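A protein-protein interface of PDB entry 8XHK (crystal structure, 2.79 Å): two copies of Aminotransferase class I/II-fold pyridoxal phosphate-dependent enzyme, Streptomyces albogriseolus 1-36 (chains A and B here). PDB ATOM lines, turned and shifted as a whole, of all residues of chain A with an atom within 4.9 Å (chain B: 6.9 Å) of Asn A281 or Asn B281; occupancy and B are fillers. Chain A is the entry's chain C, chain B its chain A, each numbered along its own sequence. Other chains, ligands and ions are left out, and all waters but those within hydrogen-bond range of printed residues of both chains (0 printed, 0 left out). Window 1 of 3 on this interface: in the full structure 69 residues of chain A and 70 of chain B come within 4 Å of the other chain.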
ATOM      1  N   LEU A  72     -27.279  24.786 -36.922  1.00  0.00           N
ATOM      2  CA  LEU A  72     -26.764  25.030 -35.579  1.00  0.00           C
ATOM      3  C   LEU A  72     -27.680  24.432 -34.519  1.00  0.00           C
ATOM      4  O   LEU A  72     -27.215  23.750 -33.599  1.00  0.00           O
ATOM      5  CB  LEU A  72     -26.593  26.529 -35.343  1.00  0.00           C
ATOM      6  CG  LEU A  72     -25.381  27.214 -35.968  1.00  0.00           C
ATOM      7  CD1 LEU A  72     -25.536  28.716 -35.859  1.00  0.00           C
ATOM      8  CD2 LEU A  72     -24.104  26.754 -35.282  1.00  0.00           C
ATOM      9  N   LEU A  76     -33.238  23.253 -30.567  1.00  0.00           N
ATOM     10  CA  LEU A  76     -33.302  24.190 -29.453  1.00  0.00           C
ATOM     11  C   LEU A  76     -34.074  25.444 -29.844  1.00  0.00           C
ATOM     12  O   LEU A  76     -34.069  25.861 -31.007  1.00  0.00           O
ATOM     13  CB  LEU A  76     -31.902  24.587 -29.001  1.00  0.00           C
ATOM     14  CG  LEU A  76     -30.876  24.933 -30.074  1.00  0.00           C
ATOM     15  CD1 LEU A  76     -30.248  26.298 -29.840  1.00  0.00           C
ATOM     16  CD2 LEU A  76     -29.814  23.873 -30.066  1.00  0.00           C
ATOM     17  N   SER A 249     -18.517  21.872 -24.455  1.00  0.00           N
ATOM     18  CA  SER A 249     -19.326  23.043 -24.153  1.00  0.00           C
ATOM     19  C   SER A 249     -20.534  22.618 -23.332  1.00  0.00           C
ATOM     20  O   SER A 249     -20.921  21.447 -23.319  1.00  0.00           O
ATOM     21  CB  SER A 249     -19.785  23.761 -25.428  1.00  0.00           C
ATOM     22  OG  SER A 249     -18.691  24.051 -26.279  1.00  0.00           O
ATOM     23  N   ARG A 279     -31.269  24.065 -26.111  1.00  0.00           N
ATOM     24  CA  ARG A 279     -30.268  23.016 -26.061  1.00  0.00           C
ATOM     25  C   ARG A 279     -28.966  23.489 -26.710  1.00  0.00           C
ATOM     26  O   ARG A 279     -28.857  24.606 -27.223  1.00  0.00           O
ATOM     27  CB  ARG A 279     -30.802  21.760 -26.745  1.00  0.00           C
ATOM     28  CG  ARG A 279     -31.866  21.018 -25.937  1.00  0.00           C
ATOM     29  CD  ARG A 279     -33.149  20.796 -26.730  1.00  0.00           C
ATOM     30  NE  ARG A 279     -34.072  19.902 -26.036  1.00  0.00           N
ATOM     31  CZ  ARG A 279     -35.312  19.645 -26.430  1.00  0.00           C
ATOM     32  NH1 ARG A 279     -35.830  20.217 -27.505  1.00  0.00           N
ATOM     33  NH2 ARG A 279     -36.053  18.794 -25.726  1.00  0.00           N
ATOM     34  N   LEU A 280     -27.963  22.615 -26.681  1.00  0.00           N
ATOM     35  CA  LEU A 280     -26.643  22.917 -27.214  1.00  0.00           C
ATOM     36  C   LEU A 280     -26.633  22.853 -28.736  1.00  0.00           C
ATOM     37  O   LEU A 280     -27.371  22.077 -29.353  1.00  0.00           O
ATOM     38  CB  LEU A 280     -25.611  21.934 -26.667  1.00  0.00           C
ATOM     39  CG  LEU A 280     -25.245  22.057 -25.193  1.00  0.00           C
ATOM     40  CD1 LEU A 280     -24.582  20.779 -24.724  1.00  0.00           C
ATOM     41  CD2 LEU A 280     -24.323  23.245 -24.998  1.00  0.00           C
ATOM     42  N   ASN A 281     -25.767  23.662 -29.342  1.00  0.00           N
ATOM     43  CA  ASN A 281     -25.650  23.645 -30.790  1.00  0.00           C
ATOM     44  C   ASN A 281     -24.911  22.388 -31.248  1.00  0.00           C
ATOM     45  O   ASN A 281     -24.276  21.682 -30.460  1.00  0.00           O
ATOM     46  CB  ASN A 281     -24.958  24.913 -31.301  1.00  0.00           C
ATOM     47  CG  ASN A 281     -23.594  25.154 -30.665  1.00  0.00           C
ATOM     48  OD1 ASN A 281     -22.929  24.228 -30.204  1.00  0.00           O
ATOM     49  ND2 ASN A 281     -23.170  26.413 -30.651  1.00  0.00           N
ATOM     50  N   THR A 282     -25.009  22.109 -32.549  1.00  0.00           N
ATOM     51  CA  THR A 282     -24.435  20.877 -33.084  1.00  0.00           C
ATOM     52  C   THR A 282     -22.936  20.725 -32.837  1.00  0.00           C
ATOM     53  O   THR A 282     -22.520  19.610 -32.474  1.00  0.00           O
ATOM     54  CB  THR A 282     -24.752  20.761 -34.583  1.00  0.00           C
ATOM     55  OG1 THR A 282     -24.591  22.036 -35.216  1.00  0.00           O
ATOM     56  CG2 THR A 282     -26.177  20.275 -34.787  1.00  0.00           C
ATOM     57  N   PRO A 283     -22.084  21.746 -33.003  1.00  0.00           N
ATOM     58  CA  PRO A 283     -20.649  21.517 -32.758  1.00  0.00           C
ATOM     59  C   PRO A 283     -20.334  21.143 -31.322  1.00  0.00           C
ATOM     60  O   PRO A 283     -19.422  20.341 -31.088  1.00  0.00           O
ATOM     61  CB  PRO A 283     -20.006  22.855 -33.148  1.00  0.00           C
ATOM     62  CG  PRO A 283     -21.094  23.846 -33.008  1.00  0.00           C
ATOM     63  CD  PRO A 283     -22.331  23.133 -33.435  1.00  0.00           C
ATOM     64  N   ALA A 284     -21.064  21.694 -30.352  1.00  0.00           N
ATOM     65  CA  ALA A 284     -20.860  21.296 -28.963  1.00  0.00           C
ATOM     66  C   ALA A 284     -21.205  19.827 -28.758  1.00  0.00           C
ATOM     67  O   ALA A 284     -20.464  19.093 -28.094  1.00  0.00           O
ATOM     68  CB  ALA A 284     -21.693  22.179 -28.035  1.00  0.00           C
ATOM     69  N   LEU A 285     -22.326  19.378 -29.330  1.00  0.00           N
ATOM     70  CA  LEU A 285     -22.735  17.986 -29.173  1.00  0.00           C
ATOM     71  C   LEU A 285     -21.732  17.037 -29.820  1.00  0.00           C
ATOM     72  O   LEU A 285     -21.404  15.989 -29.252  1.00  0.00           O
ATOM     73  CB  LEU A 285     -24.131  17.781 -29.761  1.00  0.00           C
ATOM     74  CG  LEU A 285     -25.263  18.565 -29.094  1.00  0.00           C
ATOM     75  CD1 LEU A 285     -26.548  18.416 -29.883  1.00  0.00           C
ATOM     76  CD2 LEU A 285     -25.460  18.106 -27.659  1.00  0.00           C
ATOM     77  N   ALA B  65     -15.120  30.249 -37.941  1.00  0.00           N
ATOM     78  CA  ALA B  65     -14.673  30.712 -36.632  1.00  0.00           C
ATOM     79  C   ALA B  65     -14.066  29.582 -35.813  1.00  0.00           C
ATOM     80  O   ALA B  65     -13.208  29.830 -34.958  1.00  0.00           O
ATOM     81  CB  ALA B  65     -15.834  31.352 -35.873  1.00  0.00           C
ATOM     82  N   LEU B  66     -14.487  28.341 -36.062  1.00  0.00           N
ATOM     83  CA  LEU B  66     -13.964  27.221 -35.290  1.00  0.00           C
ATOM     84  C   LEU B  66     -12.607  26.761 -35.814  1.00  0.00           C
ATOM     85  O   LEU B  66     -11.732  26.389 -35.024  1.00  0.00           O
ATOM     86  CB  LEU B  66     -14.968  26.069 -35.297  1.00  0.00           C
ATOM     87  CG  LEU B  66     -14.668  24.891 -34.372  1.00  0.00           C
ATOM     88  CD1 LEU B  66     -14.174  25.374 -33.017  1.00  0.00           C
ATOM     89  CD2 LEU B  66     -15.915  24.039 -34.209  1.00  0.00           C
ATOM     90  N   VAL B  71     -10.179  26.493 -31.092  1.00  0.00           N
ATOM     91  CA  VAL B  71     -10.671  26.217 -29.748  1.00  0.00           C
ATOM     92  C   VAL B  71     -12.173  26.468 -29.723  1.00  0.00           C
ATOM     93  O   VAL B  71     -12.711  27.246 -30.513  1.00  0.00           O
ATOM     94  CB  VAL B  71      -9.978  27.071 -28.658  1.00  0.00           C
ATOM     95  CG1 VAL B  71      -8.509  26.697 -28.524  1.00  0.00           C
ATOM     96  CG2 VAL B  71     -10.136  28.559 -28.954  1.00  0.00           C
ATOM     97  N   LEU B  72     -12.850  25.792 -28.795  1.00  0.00           N
ATOM     98  CA  LEU B  72     -14.286  25.974 -28.612  1.00  0.00           C
ATOM     99  C   LEU B  72     -14.601  27.137 -27.678  1.00  0.00           C
ATOM    100  O   LEU B  72     -15.460  27.967 -27.988  1.00  0.00           O
ATOM    101  CB  LEU B  72     -14.915  24.688 -28.074  1.00  0.00           C
ATOM    102  CG  LEU B  72     -15.356  23.661 -29.112  1.00  0.00           C
ATOM    103  CD1 LEU B  72     -15.685  22.353 -28.424  1.00  0.00           C
ATOM    104  CD2 LEU B  72     -16.556  24.179 -29.897  1.00  0.00           C
ATOM    105  N   ASN B  73     -13.923  27.205 -26.536  1.00  0.00           N
ATOM    106  CA  ASN B  73     -14.199  28.249 -25.557  1.00  0.00           C
ATOM    107  C   ASN B  73     -13.715  29.603 -26.060  1.00  0.00           C
ATOM    108  O   ASN B  73     -12.586  29.735 -26.543  1.00  0.00           O
ATOM    109  CB  ASN B  73     -13.533  27.916 -24.224  1.00  0.00           C
ATOM    110  CG  ASN B  73     -14.238  26.796 -23.481  1.00  0.00           C
ATOM    111  OD1 ASN B  73     -15.059  26.074 -24.049  1.00  0.00           O
ATOM    112  ND2 ASN B  73     -13.920  26.648 -22.200  1.00  0.00           N
ATOM    113  N   SER B  74     -14.574  30.612 -25.940  1.00  0.00           N
ATOM    114  CA  SER B  74     -14.229  31.984 -26.282  1.00  0.00           C
ATOM    115  C   SER B  74     -13.684  32.766 -25.095  1.00  0.00           C
ATOM    116  O   SER B  74     -13.296  33.928 -25.261  1.00  0.00           O
ATOM    117  CB  SER B  74     -15.452  32.708 -26.851  1.00  0.00           C
ATOM    118  OG  SER B  74     -16.491  32.801 -25.891  1.00  0.00           O
ATOM    119  N   LEU B  85     -12.790  37.171 -31.142  1.00  0.00           N
ATOM    120  CA  LEU B  85     -14.052  36.824 -31.783  1.00  0.00           C
ATOM    121  C   LEU B  85     -15.248  37.271 -30.952  1.00  0.00           C
ATOM    122  O   LEU B  85     -16.274  37.680 -31.510  1.00  0.00           O
ATOM    123  CB  LEU B  85     -14.113  35.317 -32.025  1.00  0.00           C
ATOM    124  CG  LEU B  85     -15.270  34.796 -32.874  1.00  0.00           C
ATOM    125  CD1 LEU B  85     -15.087  35.192 -34.330  1.00  0.00           C
ATOM    126  CD2 LEU B  85     -15.379  33.289 -32.734  1.00  0.00           C
ATOM    127  N   ALA B 248     -28.751  32.018 -35.091  1.00  0.00           N
ATOM    128  CA  ALA B 248     -27.491  31.681 -34.438  1.00  0.00           C
ATOM    129  C   ALA B 248     -27.721  30.925 -33.134  1.00  0.00           C
ATOM    130  O   ALA B 248     -28.581  30.042 -33.064  1.00  0.00           O
ATOM    131  CB  ALA B 248     -26.675  32.947 -34.178  1.00  0.00           C
ATOM    132  N   SER B 249     -26.954  31.264 -32.099  1.00  0.00           N
ATOM    133  CA  SER B 249     -27.047  30.597 -30.810  1.00  0.00           C
ATOM    134  C   SER B 249     -26.964  31.628 -29.694  1.00  0.00           C
ATOM    135  O   SER B 249     -26.462  32.739 -29.882  1.00  0.00           O
ATOM    136  CB  SER B 249     -25.941  29.548 -30.628  1.00  0.00           C
ATOM    137  OG  SER B 249     -25.995  28.562 -31.642  1.00  0.00           O
ATOM    138  N   GLY B 250     -27.461  31.241 -28.524  1.00  0.00           N
ATOM    139  CA  GLY B 250     -27.335  32.058 -27.338  1.00  0.00           C
ATOM    140  C   GLY B 250     -28.327  33.207 -27.279  1.00  0.00           C
ATOM    141  O   GLY B 250     -29.234  33.349 -28.105  1.00  0.00           O
ATOM    142  N   GLN B 278     -20.333  29.993 -18.448  1.00  0.00           N
ATOM    143  CA  GLN B 278     -19.514  29.969 -19.652  1.00  0.00           C
ATOM    144  C   GLN B 278     -20.128  30.831 -20.748  1.00  0.00           C
ATOM    145  O   GLN B 278     -21.346  31.011 -20.825  1.00  0.00           O
ATOM    146  CB  GLN B 278     -19.341  28.536 -20.155  1.00  0.00           C
ATOM    147  CG  GLN B 278     -20.645  27.811 -20.429  1.00  0.00           C
ATOM    148  CD  GLN B 278     -20.429  26.373 -20.853  1.00  0.00           C
ATOM    149  OE1 GLN B 278     -20.131  26.095 -22.014  1.00  0.00           O
ATOM    150  NE2 GLN B 278     -20.576  25.449 -19.908  1.00  0.00           N
ATOM    151  N   ARG B 279     -19.263  31.365 -21.600  1.00  0.00           N
ATOM    152  CA  ARG B 279     -19.685  32.212 -22.701  1.00  0.00           C
ATOM    153  C   ARG B 279     -19.850  31.378 -23.970  1.00  0.00           C
ATOM    154  O   ARG B 279     -19.425  30.223 -24.045  1.00  0.00           O
ATOM    155  CB  ARG B 279     -18.679  33.347 -22.898  1.00  0.00           C
ATOM    156  CG  ARG B 279     -18.387  34.096 -21.602  1.00  0.00           C
ATOM    157  CD  ARG B 279     -17.384  35.224 -21.778  1.00  0.00           C
ATOM    158  NE  ARG B 279     -17.002  35.798 -20.493  1.00  0.00           N
ATOM    159  CZ  ARG B 279     -16.172  36.823 -20.342  1.00  0.00           C
ATOM    160  NH1 ARG B 279     -15.628  37.430 -21.383  1.00  0.00           N
ATOM    161  NH2 ARG B 279     -15.881  37.247 -19.115  1.00  0.00           N
ATOM    162  N   LEU B 280     -20.498  31.977 -24.968  1.00  0.00           N
ATOM    163  CA  LEU B 280     -20.800  31.265 -26.204  1.00  0.00           C
ATOM    164  C   LEU B 280     -19.528  30.745 -26.858  1.00  0.00           C
ATOM    165  O   LEU B 280     -18.495  31.417 -26.867  1.00  0.00           O
ATOM    166  CB  LEU B 280     -21.544  32.184 -27.171  1.00  0.00           C
ATOM    167  CG  LEU B 280     -23.004  32.455 -26.820  1.00  0.00           C
ATOM    168  CD1 LEU B 280     -23.555  33.563 -27.688  1.00  0.00           C
ATOM    169  CD2 LEU B 280     -23.822  31.186 -26.982  1.00  0.00           C
ATOM    170  N   ASN B 281     -19.607  29.534 -27.404  1.00  0.00           N
ATOM    171  CA  ASN B 281     -18.447  28.967 -28.067  1.00  0.00           C
ATOM    172  C   ASN B 281     -18.182  29.695 -29.384  1.00  0.00           C
ATOM    173  O   ASN B 281     -18.972  30.528 -29.840  1.00  0.00           O
ATOM    174  CB  ASN B 281     -18.626  27.462 -28.288  1.00  0.00           C
ATOM    175  CG  ASN B 281     -19.878  27.116 -29.075  1.00  0.00           C
ATOM    176  OD1 ASN B 281     -20.445  27.951 -29.779  1.00  0.00           O
ATOM    177  ND2 ASN B 281     -20.309  25.866 -28.962  1.00  0.00           N
ATOM    178  N   THR B 282     -17.046  29.369 -29.997  1.00  0.00           N
ATOM    179  CA  THR B 282     -16.613  30.100 -31.187  1.00  0.00           C
ATOM    180  C   THR B 282     -17.588  29.998 -32.355  1.00  0.00           C
ATOM    181  O   THR B 282     -17.904  31.045 -32.949  1.00  0.00           O
ATOM    182  CB  THR B 282     -15.202  29.651 -31.587  1.00  0.00           C
ATOM    183  OG1 THR B 282     -15.071  28.235 -31.419  1.00  0.00           O
ATOM    184  CG2 THR B 282     -14.163  30.353 -30.725  1.00  0.00           C
ATOM    185  N   PRO B 283     -18.101  28.822 -32.744  1.00  0.00           N
ATOM    186  CA  PRO B 283     -19.015  28.799 -33.899  1.00  0.00           C
ATOM    187  C   PRO B 283     -20.283  29.604 -33.677  1.00  0.00           C
ATOM    188  O   PRO B 283     -20.796  30.204 -34.629  1.00  0.00           O
ATOM    189  CB  PRO B 283     -19.313  27.304 -34.082  1.00  0.00           C
ATOM    190  CG  PRO B 283     -19.065  26.707 -32.751  1.00  0.00           C
ATOM    191  CD  PRO B 283     -17.921  27.471 -32.180  1.00  0.00           C
ATOM    192  N   ALA B 284     -20.798  29.643 -32.446  1.00  0.00           N
ATOM    193  CA  ALA B 284     -21.943  30.496 -32.150  1.00  0.00           C
ATOM    194  C   ALA B 284     -21.605  31.965 -32.363  1.00  0.00           C
ATOM    195  O   ALA B 284     -22.419  32.726 -32.899  1.00  0.00           O
ATOM    196  CB  ALA B 284     -22.416  30.263 -30.717  1.00  0.00           C
ATOM    197  N   LEU B 285     -20.406  32.381 -31.947  1.00  0.00           N
ATOM    198  CA  LEU B 285     -19.996  33.766 -32.142  1.00  0.00           C
ATOM    199  C   LEU B 285     -19.764  34.069 -33.616  1.00  0.00           C
ATOM    200  O   LEU B 285     -20.145  35.141 -34.101  1.00  0.00           O
ATOM    201  CB  LEU B 285     -18.741  34.061 -31.326  1.00  0.00           C
ATOM    202  CG  LEU B 285     -18.924  33.984 -29.811  1.00  0.00           C
ATOM    203  CD1 LEU B 285     -17.618  34.279 -29.117  1.00  0.00           C
ATOM    204  CD2 LEU B 285     -20.005  34.946 -29.350  1.00  0.00           C
ATOM    205  N   GLY B 286     -19.139  33.141 -34.343  1.00  0.00           N
ATOM    206  CA  GLY B 286     -18.972  33.331 -35.772  1.00  0.00           C
ATOM    207  C   GLY B 286     -20.293  33.468 -36.500  1.00  0.00           C
ATOM    208  O   GLY B 286     -20.402  34.234 -37.463  1.00  0.00           O
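Ser A249 touches Asn B281, and with the chains exchanged Asn A281 touches Ser B249.
Asn A281 touches its own counterpart, Asn B281.
Asn A281 touches Ala B284, but with the chains exchanged Ala A284 does not touch Asn B281 (4.05 Å).
Pro B283 touches its own counterpart, Pro A283.
Printed residues of chain B within 4 Å of Asn A281: Ser B249 (3.7 Å), Asn B281 (3.2 Å) and Ala B284 (3.9 Å).
Of chain A, only Ser A249 (3.6 Å) and Asn A281 (3.2 Å) come within 4 Å of Asn B281.
Printed residues of chain B within 4 Å of Leu A72: Ala B248 (3.8 Å).
Of the printed residues of chain A, Ala B284 touches Asn A281.
Of the printed residues of chain A, Pro B283 touches Pro A283.
Leu B66 touches none of the printed residues of chain A.
Leu A76 touches none of the printed residues of chain B.
The nearest residue of chain B that does not touch Asn A281 is Pro B283 (4.6 Å).
The nearest residue of chain A that does not touch Asn B281 is Ala A284 (4.05 Å).
The backbone NH (N) of Thr A282 sits at hydrogen-bond distance from the backbone carbonyl oxygen (O) of Leu A72.
The side-chain amide oxygen (OD1) of Asn A281 is in hydrogen-bond range of the backbone NH (N) of Ala A284, 3.1 Å away.
N of Ala B284 lies within hydrogen-bond range of OD1 of Asn B281.
Among the printed residues, merely in contact across the chains: Pro A283 with Pro B283 (3.5 Å), Ser A249 with Asn B281 (3.6 Å), Asn A281 with Ser B249 (3.7 Å), Ser A249 with Gln B278 (3.7 Å), Leu A72 with Ala B248 (3.8 Å) and Asn A281 with Ala B284 (3.9 Å).
ND2 of Asn A281 sits at hydrogen-bond distance from OD1 of Asn B281, 3.2 Å away.
Of the 19 printed residues of chain B, 6 touch a printed residue of chain A.
Hydrophobic or aromatic side chains of chain B within 4 Å of the printed part of chain A: Pro B283 and Ala B284.
Printed residues of chain A that touch a printed residue of chain B: Leu A72, Ser A249, Asn A281 and Pro A283.
Hydrophobic or aromatic side chains of chain A that line the printed part of chain B: Leu A72 and Pro A283.
Among the printed residues, 7 pairs touch across the chains.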
